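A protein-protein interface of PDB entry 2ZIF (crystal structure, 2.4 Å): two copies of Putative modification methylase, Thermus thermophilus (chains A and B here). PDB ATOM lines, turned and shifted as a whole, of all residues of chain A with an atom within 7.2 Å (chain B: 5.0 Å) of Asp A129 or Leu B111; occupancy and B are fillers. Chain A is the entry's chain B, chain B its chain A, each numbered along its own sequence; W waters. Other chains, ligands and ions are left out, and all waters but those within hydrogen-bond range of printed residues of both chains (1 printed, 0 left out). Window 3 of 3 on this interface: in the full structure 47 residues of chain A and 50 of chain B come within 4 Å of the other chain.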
ATOM      1  N   PHE A  84     -13.321   8.500  -9.665  1.00  0.00           N
ATOM      2  CA  PHE A  84     -13.972   9.627 -10.323  1.00  0.00           C
ATOM      3  C   PHE A  84     -14.565  10.621  -9.330  1.00  0.00           C
ATOM      4  O   PHE A  84     -14.642  11.816  -9.602  1.00  0.00           O
ATOM      5  CB  PHE A  84     -15.062   9.130 -11.274  1.00  0.00           C
ATOM      6  CG  PHE A  84     -15.657  10.213 -12.118  1.00  0.00           C
ATOM      7  CD1 PHE A  84     -16.657  11.036 -11.617  1.00  0.00           C
ATOM      8  CD2 PHE A  84     -15.180  10.448 -13.399  1.00  0.00           C
ATOM      9  CE1 PHE A  84     -17.165  12.078 -12.378  1.00  0.00           C
ATOM     10  CE2 PHE A  84     -15.687  11.493 -14.169  1.00  0.00           C
ATOM     11  CZ  PHE A  84     -16.679  12.306 -13.654  1.00  0.00           C
ATOM     12  N   ARG A  92      -6.804  13.382 -13.011  1.00  0.00           N
ATOM     13  CA  ARG A  92      -6.941  12.210 -13.857  1.00  0.00           C
ATOM     14  C   ARG A  92      -6.553  10.878 -13.270  1.00  0.00           C
ATOM     15  O   ARG A  92      -5.826  10.769 -12.271  1.00  0.00           O
ATOM     16  CB  ARG A  92      -6.196  12.405 -15.180  1.00  0.00           C
ATOM     17  CG  ARG A  92      -4.681  12.432 -15.072  1.00  0.00           C
ATOM     18  CD  ARG A  92      -4.039  12.582 -16.454  1.00  0.00           C
ATOM     19  NE  ARG A  92      -4.168  13.931 -17.016  1.00  0.00           N
ATOM     20  CZ  ARG A  92      -3.813  14.255 -18.256  1.00  0.00           C
ATOM     21  NH1 ARG A  92      -3.313  13.327 -19.077  1.00  0.00           N
ATOM     22  NH2 ARG A  92      -3.935  15.508 -18.676  1.00  0.00           N
ATOM     23  N   CYS A 123     -14.664   3.275 -18.730  1.00  0.00           N
ATOM     24  CA  CYS A 123     -14.400   4.499 -17.982  1.00  0.00           C
ATOM     25  C   CYS A 123     -15.255   5.652 -18.504  1.00  0.00           C
ATOM     26  O   CYS A 123     -15.545   6.605 -17.779  1.00  0.00           O
ATOM     27  CB  CYS A 123     -12.914   4.867 -18.049  1.00  0.00           C
ATOM     28  SG  CYS A 123     -11.861   3.993 -16.846  1.00  0.00           S
ATOM     29  N   ARG A 124     -15.659   5.568 -19.766  1.00  0.00           N
ATOM     30  CA  ARG A 124     -16.486   6.607 -20.364  1.00  0.00           C
ATOM     31  C   ARG A 124     -17.867   6.530 -19.727  1.00  0.00           C
ATOM     32  O   ARG A 124     -18.418   7.535 -19.288  1.00  0.00           O
ATOM     33  CB  ARG A 124     -16.602   6.393 -21.874  1.00  0.00           C
ATOM     34  CG  ARG A 124     -17.466   7.431 -22.576  1.00  0.00           C
ATOM     35  CD  ARG A 124     -17.496   7.219 -24.087  1.00  0.00           C
ATOM     36  NE  ARG A 124     -18.117   5.949 -24.452  1.00  0.00           N
ATOM     37  CZ  ARG A 124     -17.528   5.025 -25.206  1.00  0.00           C
ATOM     38  NH1 ARG A 124     -16.304   5.237 -25.668  1.00  0.00           N
ATOM     39  NH2 ARG A 124     -18.158   3.894 -25.507  1.00  0.00           N
ATOM     40  N   LEU A 126     -18.571   5.765 -17.072  1.00  0.00           N
ATOM     41  CA  LEU A 126     -18.477   6.256 -15.711  1.00  0.00           C
ATOM     42  C   LEU A 126     -18.344   7.777 -15.679  1.00  0.00           C
ATOM     43  O   LEU A 126     -18.282   8.379 -14.610  1.00  0.00           O
ATOM     44  CB  LEU A 126     -17.293   5.600 -14.989  1.00  0.00           C
ATOM     45  CG  LEU A 126     -17.313   4.067 -14.894  1.00  0.00           C
ATOM     46  CD1 LEU A 126     -16.251   3.610 -13.912  1.00  0.00           C
ATOM     47  CD2 LEU A 126     -18.673   3.582 -14.419  1.00  0.00           C
ATOM     48  N   GLY A 127     -18.294   8.398 -16.852  1.00  0.00           N
ATOM     49  CA  GLY A 127     -18.186   9.844 -16.904  1.00  0.00           C
ATOM     50  C   GLY A 127     -16.837  10.430 -17.292  1.00  0.00           C
ATOM     51  O   GLY A 127     -16.745  11.621 -17.596  1.00  0.00           O
ATOM     52  N   PHE A 128     -15.790   9.609 -17.290  1.00  0.00           N
ATOM     53  CA  PHE A 128     -14.452  10.081 -17.642  1.00  0.00           C
ATOM     54  C   PHE A 128     -14.322  10.582 -19.076  1.00  0.00           C
ATOM     55  O   PHE A 128     -15.011  10.109 -19.975  1.00  0.00           O
ATOM     56  CB  PHE A 128     -13.422   8.962 -17.439  1.00  0.00           C
ATOM     57  CG  PHE A 128     -13.073   8.706 -16.009  1.00  0.00           C
ATOM     58  CD1 PHE A 128     -12.246   9.575 -15.319  1.00  0.00           C
ATOM     59  CD2 PHE A 128     -13.544   7.575 -15.360  1.00  0.00           C
ATOM     60  CE1 PHE A 128     -11.890   9.320 -14.017  1.00  0.00           C
ATOM     61  CE2 PHE A 128     -13.186   7.309 -14.043  1.00  0.00           C
ATOM     62  CZ  PHE A 128     -12.362   8.178 -13.372  1.00  0.00           C
ATOM     63  N   ASP A 129     -13.439  11.555 -19.267  1.00  0.00           N
ATOM     64  CA  ASP A 129     -13.146  12.076 -20.592  1.00  0.00           C
ATOM     65  C   ASP A 129     -11.929  11.269 -21.022  1.00  0.00           C
ATOM     66  O   ASP A 129     -10.928  11.213 -20.300  1.00  0.00           O
ATOM     67  CB  ASP A 129     -12.748  13.556 -20.552  1.00  0.00           C
ATOM     68  CG  ASP A 129     -13.917  14.485 -20.817  1.00  0.00           C
ATOM     69  OD1 ASP A 129     -14.773  14.136 -21.657  1.00  0.00           O
ATOM     70  OD2 ASP A 129     -13.966  15.569 -20.199  1.00  0.00           O
ATOM     71  N   ASN A 130     -12.003  10.636 -22.181  1.00  0.00           N
ATOM     72  CA  ASN A 130     -10.868   9.859 -22.639  1.00  0.00           C
ATOM     73  C   ASN A 130      -9.815  10.734 -23.298  1.00  0.00           C
ATOM     74  O   ASN A 130     -10.123  11.560 -24.156  1.00  0.00           O
ATOM     75  CB  ASN A 130     -11.298   8.791 -23.634  1.00  0.00           C
ATOM     76  CG  ASN A 130     -10.125   7.983 -24.148  1.00  0.00           C
ATOM     77  OD1 ASN A 130      -9.569   7.142 -23.435  1.00  0.00           O
ATOM     78  ND2 ASN A 130      -9.731   8.247 -25.386  1.00  0.00           N
ATOM     79  N   LEU A 131      -8.573  10.544 -22.874  1.00  0.00           N
ATOM     80  CA  LEU A 131      -7.443  11.260 -23.434  1.00  0.00           C
ATOM     81  C   LEU A 131      -6.584  10.220 -24.164  1.00  0.00           C
ATOM     82  O   LEU A 131      -6.769   9.009 -23.980  1.00  0.00           O
ATOM     83  CB  LEU A 131      -6.634  11.932 -22.316  1.00  0.00           C
ATOM     84  CG  LEU A 131      -6.899  13.420 -22.068  1.00  0.00           C
ATOM     85  CD1 LEU A 131      -8.404  13.674 -21.986  1.00  0.00           C
ATOM     86  CD2 LEU A 131      -6.209  13.865 -20.786  1.00  0.00           C
ATOM     87  N   ASN A 132      -5.656  10.681 -24.997  1.00  0.00           N
ATOM     88  CA  ASN A 132      -4.802   9.749 -25.714  1.00  0.00           C
ATOM     89  C   ASN A 132      -3.884   8.972 -24.776  1.00  0.00           C
ATOM     90  O   ASN A 132      -3.284   9.529 -23.864  1.00  0.00           O
ATOM     91  CB  ASN A 132      -3.959  10.481 -26.760  1.00  0.00           C
ATOM     92  CG  ASN A 132      -4.517  10.327 -28.152  1.00  0.00           C
ATOM     93  OD1 ASN A 132      -5.310   9.423 -28.409  1.00  0.00           O
ATOM     94  ND2 ASN A 132      -4.099  11.194 -29.063  1.00  0.00           N
ATOM     95  N   MET A 172      -5.274   7.188 -20.031  1.00  0.00           N
ATOM     96  CA  MET A 172      -5.470   8.495 -19.400  1.00  0.00           C
ATOM     97  C   MET A 172      -6.957   8.877 -19.360  1.00  0.00           C
ATOM     98  O   MET A 172      -7.573   9.147 -20.394  1.00  0.00           O
ATOM     99  CB  MET A 172      -4.705   9.571 -20.181  1.00  0.00           C
ATOM    100  CG  MET A 172      -3.252   9.231 -20.483  1.00  0.00           C
ATOM    101  SD  MET A 172      -2.123   9.696 -19.170  1.00  0.00           S
ATOM    102  CE  MET A 172      -0.700  10.074 -20.123  1.00  0.00           C
ATOM    103  N   GLN A 173      -7.521   8.904 -18.157  1.00  0.00           N
ATOM    104  CA  GLN A 173      -8.920   9.260 -17.977  1.00  0.00           C
ATOM    105  C   GLN A 173      -9.032  10.519 -17.132  1.00  0.00           C
ATOM    106  O   GLN A 173      -8.722  10.516 -15.938  1.00  0.00           O
ATOM    107  CB  GLN A 173      -9.685   8.101 -17.333  1.00  0.00           C
ATOM    108  CG  GLN A 173     -10.455   7.265 -18.333  1.00  0.00           C
ATOM    109  CD  GLN A 173      -9.570   6.686 -19.403  1.00  0.00           C
ATOM    110  OE1 GLN A 173      -8.661   5.911 -19.108  1.00  0.00           O
ATOM    111  NE2 GLN A 173      -9.824   7.049 -20.655  1.00  0.00           N
ATOM    112  N   ARG A 174      -9.469  11.595 -17.778  1.00  0.00           N
ATOM    113  CA  ARG A 174      -9.611  12.898 -17.141  1.00  0.00           C
ATOM    114  C   ARG A 174     -11.040  13.163 -16.660  1.00  0.00           C
ATOM    115  O   ARG A 174     -12.017  12.909 -17.374  1.00  0.00           O
ATOM    116  CB  ARG A 174      -9.190  13.997 -18.131  1.00  0.00           C
ATOM    117  CG  ARG A 174      -9.071  15.399 -17.545  1.00  0.00           C
ATOM    118  CD  ARG A 174      -9.479  16.460 -18.562  1.00  0.00           C
ATOM    119  NE  ARG A 174      -8.433  16.774 -19.535  1.00  0.00           N
ATOM    120  CZ  ARG A 174      -8.663  17.316 -20.732  1.00  0.00           C
ATOM    121  NH1 ARG A 174      -7.652  17.575 -21.557  1.00  0.00           N
ATOM    122  NH2 ARG A 174      -9.906  17.578 -21.121  1.00  0.00           N
ATOM    123  N   LYS A 175     -11.153  13.672 -15.439  1.00  0.00           N
ATOM    124  CA  LYS A 175     -12.455  14.005 -14.873  1.00  0.00           C
ATOM    125  C   LYS A 175     -12.807  15.410 -15.323  1.00  0.00           C
ATOM    126  O   LYS A 175     -12.102  16.362 -14.997  1.00  0.00           O
ATOM    127  CB  LYS A 175     -12.427  13.984 -13.344  1.00  0.00           C
ATOM    128  CG  LYS A 175     -13.687  14.581 -12.710  1.00  0.00           C
ATOM    129  CD  LYS A 175     -13.741  14.311 -11.219  1.00  0.00           C
ATOM    130  CE  LYS A 175     -15.075  14.734 -10.630  1.00  0.00           C
ATOM    131  NZ  LYS A 175     -15.157  14.396  -9.181  1.00  0.00           N
ATOM    132  N   PRO A 176     -13.901  15.557 -16.077  1.00  0.00           N
ATOM    133  CA  PRO A 176     -14.313  16.880 -16.551  1.00  0.00           C
ATOM    134  C   PRO A 176     -14.740  17.734 -15.359  1.00  0.00           C
ATOM    135  O   PRO A 176     -15.014  17.211 -14.280  1.00  0.00           O
ATOM    136  CB  PRO A 176     -15.478  16.559 -17.476  1.00  0.00           C
ATOM    137  CG  PRO A 176     -16.115  15.382 -16.780  1.00  0.00           C
ATOM    138  CD  PRO A 176     -14.918  14.537 -16.395  1.00  0.00           C
ATOM    139  N   GLY A 177     -14.790  19.046 -15.548  1.00  0.00           N
ATOM    140  CA  GLY A 177     -15.198  19.911 -14.459  1.00  0.00           C
ATOM    141  C   GLY A 177     -14.466  21.233 -14.456  1.00  0.00           C
ATOM    142  O   GLY A 177     -14.682  22.071 -13.578  1.00  0.00           O
ATOM    143  N   VAL B 100     -10.232   9.299 -32.777  1.00  0.00           N
ATOM    144  CA  VAL B 100     -10.758  10.623 -33.109  1.00  0.00           C
ATOM    145  C   VAL B 100     -10.626  11.696 -32.030  1.00  0.00           C
ATOM    146  O   VAL B 100     -11.366  11.689 -31.048  1.00  0.00           O
ATOM    147  CB  VAL B 100     -12.249  10.517 -33.485  1.00  0.00           C
ATOM    148  CG1 VAL B 100     -12.744  11.846 -34.036  1.00  0.00           C
ATOM    149  CG2 VAL B 100     -12.450   9.383 -34.489  1.00  0.00           C
ATOM    150  N   ALA B 101      -9.709  12.635 -32.230  1.00  0.00           N
ATOM    151  CA  ALA B 101      -9.506  13.709 -31.266  1.00  0.00           C
ATOM    152  C   ALA B 101     -10.276  14.993 -31.611  1.00  0.00           C
ATOM    153  O   ALA B 101     -10.470  15.324 -32.785  1.00  0.00           O
ATOM    154  CB  ALA B 101      -8.023  14.014 -31.145  1.00  0.00           C
ATOM    155  N   VAL B 102     -10.712  15.704 -30.573  1.00  0.00           N
ATOM    156  CA  VAL B 102     -11.441  16.968 -30.723  1.00  0.00           C
ATOM    157  C   VAL B 102     -11.063  17.919 -29.575  1.00  0.00           C
ATOM    158  O   VAL B 102     -11.363  17.654 -28.409  1.00  0.00           O
ATOM    159  CB  VAL B 102     -12.986  16.740 -30.734  1.00  0.00           C
ATOM    160  CG1 VAL B 102     -13.365  15.812 -31.881  1.00  0.00           C
ATOM    161  CG2 VAL B 102     -13.453  16.155 -29.406  1.00  0.00           C
ATOM    162  N   ALA B 103     -10.395  19.024 -29.908  1.00  0.00           N
ATOM    163  CA  ALA B 103      -9.965  19.995 -28.898  1.00  0.00           C
ATOM    164  C   ALA B 103     -10.884  21.217 -28.779  1.00  0.00           C
ATOM    165  O   ALA B 103     -12.111  21.090 -28.800  1.00  0.00           O
ATOM    166  CB  ALA B 103      -8.530  20.446 -29.189  1.00  0.00           C
ATOM    167  N   ARG B 109     -13.477  21.634 -24.790  1.00  0.00           N
ATOM    168  CA  ARG B 109     -12.654  20.824 -23.897  1.00  0.00           C
ATOM    169  C   ARG B 109     -12.052  19.672 -24.697  1.00  0.00           C
ATOM    170  O   ARG B 109     -12.776  18.875 -25.292  1.00  0.00           O
ATOM    171  CB  ARG B 109     -13.499  20.262 -22.748  1.00  0.00           C
ATOM    172  CG  ARG B 109     -14.643  19.372 -23.210  1.00  0.00           C
ATOM    173  CD  ARG B 109     -15.247  18.551 -22.075  1.00  0.00           C
ATOM    174  NE  ARG B 109     -16.285  17.653 -22.581  1.00  0.00           N
ATOM    175  CZ  ARG B 109     -16.923  16.744 -21.848  1.00  0.00           C
ATOM    176  NH1 ARG B 109     -17.851  15.977 -22.408  1.00  0.00           N
ATOM    177  NH2 ARG B 109     -16.637  16.598 -20.563  1.00  0.00           N
ATOM    178  N   HIS B 110     -10.727  19.592 -24.720  1.00  0.00           N
ATOM    179  CA  HIS B 110     -10.055  18.527 -25.456  1.00  0.00           C
ATOM    180  C   HIS B 110     -10.639  17.166 -25.122  1.00  0.00           C
ATOM    181  O   HIS B 110     -10.811  16.815 -23.954  1.00  0.00           O
ATOM    182  CB  HIS B 110      -8.563  18.499 -25.142  1.00  0.00           C
ATOM    183  CG  HIS B 110      -7.864  17.299 -25.698  1.00  0.00           C
ATOM    184  ND1 HIS B 110      -7.691  17.099 -27.050  1.00  0.00           N
ATOM    185  CD2 HIS B 110      -7.329  16.216 -25.088  1.00  0.00           C
ATOM    186  CE1 HIS B 110      -7.080  15.945 -27.249  1.00  0.00           C
ATOM    187  NE2 HIS B 110      -6.849  15.389 -26.074  1.00  0.00           N
ATOM    188  N   LEU B 111     -10.935  16.394 -26.155  1.00  0.00           N
ATOM    189  CA  LEU B 111     -11.487  15.068 -25.956  1.00  0.00           C
ATOM    190  C   LEU B 111     -11.150  14.118 -27.098  1.00  0.00           C
ATOM    191  O   LEU B 111     -11.225  14.480 -28.273  1.00  0.00           O
ATOM    192  CB  LEU B 111     -13.004  15.137 -25.794  1.00  0.00           C
ATOM    193  CG  LEU B 111     -13.627  13.753 -25.603  1.00  0.00           C
ATOM    194  CD1 LEU B 111     -12.993  13.089 -24.381  1.00  0.00           C
ATOM    195  CD2 LEU B 111     -15.138  13.874 -25.453  1.00  0.00           C
ATOM    196  N   VAL B 112     -10.788  12.894 -26.739  1.00  0.00           N
ATOM    197  CA  VAL B 112     -10.451  11.892 -27.731  1.00  0.00           C
ATOM    198  C   VAL B 112     -11.430  10.735 -27.656  1.00  0.00           C
ATOM    199  O   VAL B 112     -11.639  10.171 -26.585  1.00  0.00           O
ATOM    200  CB  VAL B 112      -9.026  11.333 -27.503  1.00  0.00           C
ATOM    201  CG1 VAL B 112      -8.668  10.352 -28.601  1.00  0.00           C
ATOM    202  CG2 VAL B 112      -8.023  12.463 -27.468  1.00  0.00           C
ATOM    203  N   PHE B 113     -12.045  10.400 -28.786  1.00  0.00           N
ATOM    204  CA  PHE B 113     -12.962   9.264 -28.848  1.00  0.00           C
ATOM    205  C   PHE B 113     -12.114   8.027 -29.120  1.00  0.00           C
ATOM    206  O   PHE B 113     -11.467   7.932 -30.162  1.00  0.00           O
ATOM    207  CB  PHE B 113     -13.984   9.455 -29.968  1.00  0.00           C
ATOM    208  CG  PHE B 113     -15.144  10.305 -29.572  1.00  0.00           C
ATOM    209  CD1 PHE B 113     -16.125   9.801 -28.729  1.00  0.00           C
ATOM    210  CD2 PHE B 113     -15.234  11.625 -29.999  1.00  0.00           C
ATOM    211  CE1 PHE B 113     -17.182  10.603 -28.312  1.00  0.00           C
ATOM    212  CE2 PHE B 113     -16.281  12.435 -29.592  1.00  0.00           C
ATOM    213  CZ  PHE B 113     -17.260  11.923 -28.744  1.00  0.00           C
HETATM  214  O   HOH W   1      -5.155  13.313 -25.622  1.00  0.00           O
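Water W1 bridges a ring nitrogen (NE2) of His B110 (2.7 Å) and the backbone NH (N) of Asn A132 (2.8 Å).
Among the printed residues, pairs that only touch across the chains: Asn A130 with Leu B111 (3.3 Å), Pro A176 with Arg B109 (3.3 Å), Asp A129 with Leu B111 (3.4 Å) and Asn A132 with Val B112 (3.5 Å).
Of the 17 printed residues of chain A, 5 touch a printed residue of chain B. Hydrophobic or aromatic side chains of chain A that line the printed part of chain B: Pro A176. Among the printed residues, Asp or Glu carboxylates within 4 Å of a Lys or Arg side-chain nitrogen of the other chain: Asp A129 with Arg B109 (2.9 Å).
No position is printed for both chains. Of the 7 pairs that touch across the chains among the printed residues, none has its exchanged pair printed and touching as well.
The backbone carbonyl oxygen of Arg A174 lies within hydrogen-bond range of the backbone NH of Asp A129 (2.7 Å). The backbone NH of Leu B111 sits at hydrogen-bond distance from the backbone carbonyl oxygen of Val B102, at 2.6 Å. OD1 of Asn A130 lies within hydrogen-bond range of NE2 of Gln A173 (2.8 Å).
Of the printed residues of chain B, Asp A129 touches Arg B109 (2.9 Å) and Leu B111 (3.4 Å). Leu B111 touches two residues of chain A. Printed residues of chain B within 4 Å of Asn A132: Val B112. Of the printed residues of chain A, Arg B109 touches Asp A129 (2.9 Å) and Pro A176 (3.3 Å). Of the printed residues of chain A, His B110 touches Arg A174. The nearest printed residue of chain B that does not touch Asp A129 is His B110 (5.0 Å). The nearest residue of chain A that does not touch Leu B111 is Leu A131 (5.2 Å). The nearest printed residue of chain A that does not touch Arg B109 is Arg A174 (4.7 Å).
NH2 of Arg B109 is in salt-bridge range of OD2 of Asp A129. The backbone carbonyl oxygen of Val B112 lies within hydrogen-bond range of the side-chain amide nitrogen of Asn A130. The guanidinium group (NH2) of Arg A174 is in hydrogen-bond range of the backbone carbonyl oxygen (O) of His B110 (3.1 Å).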
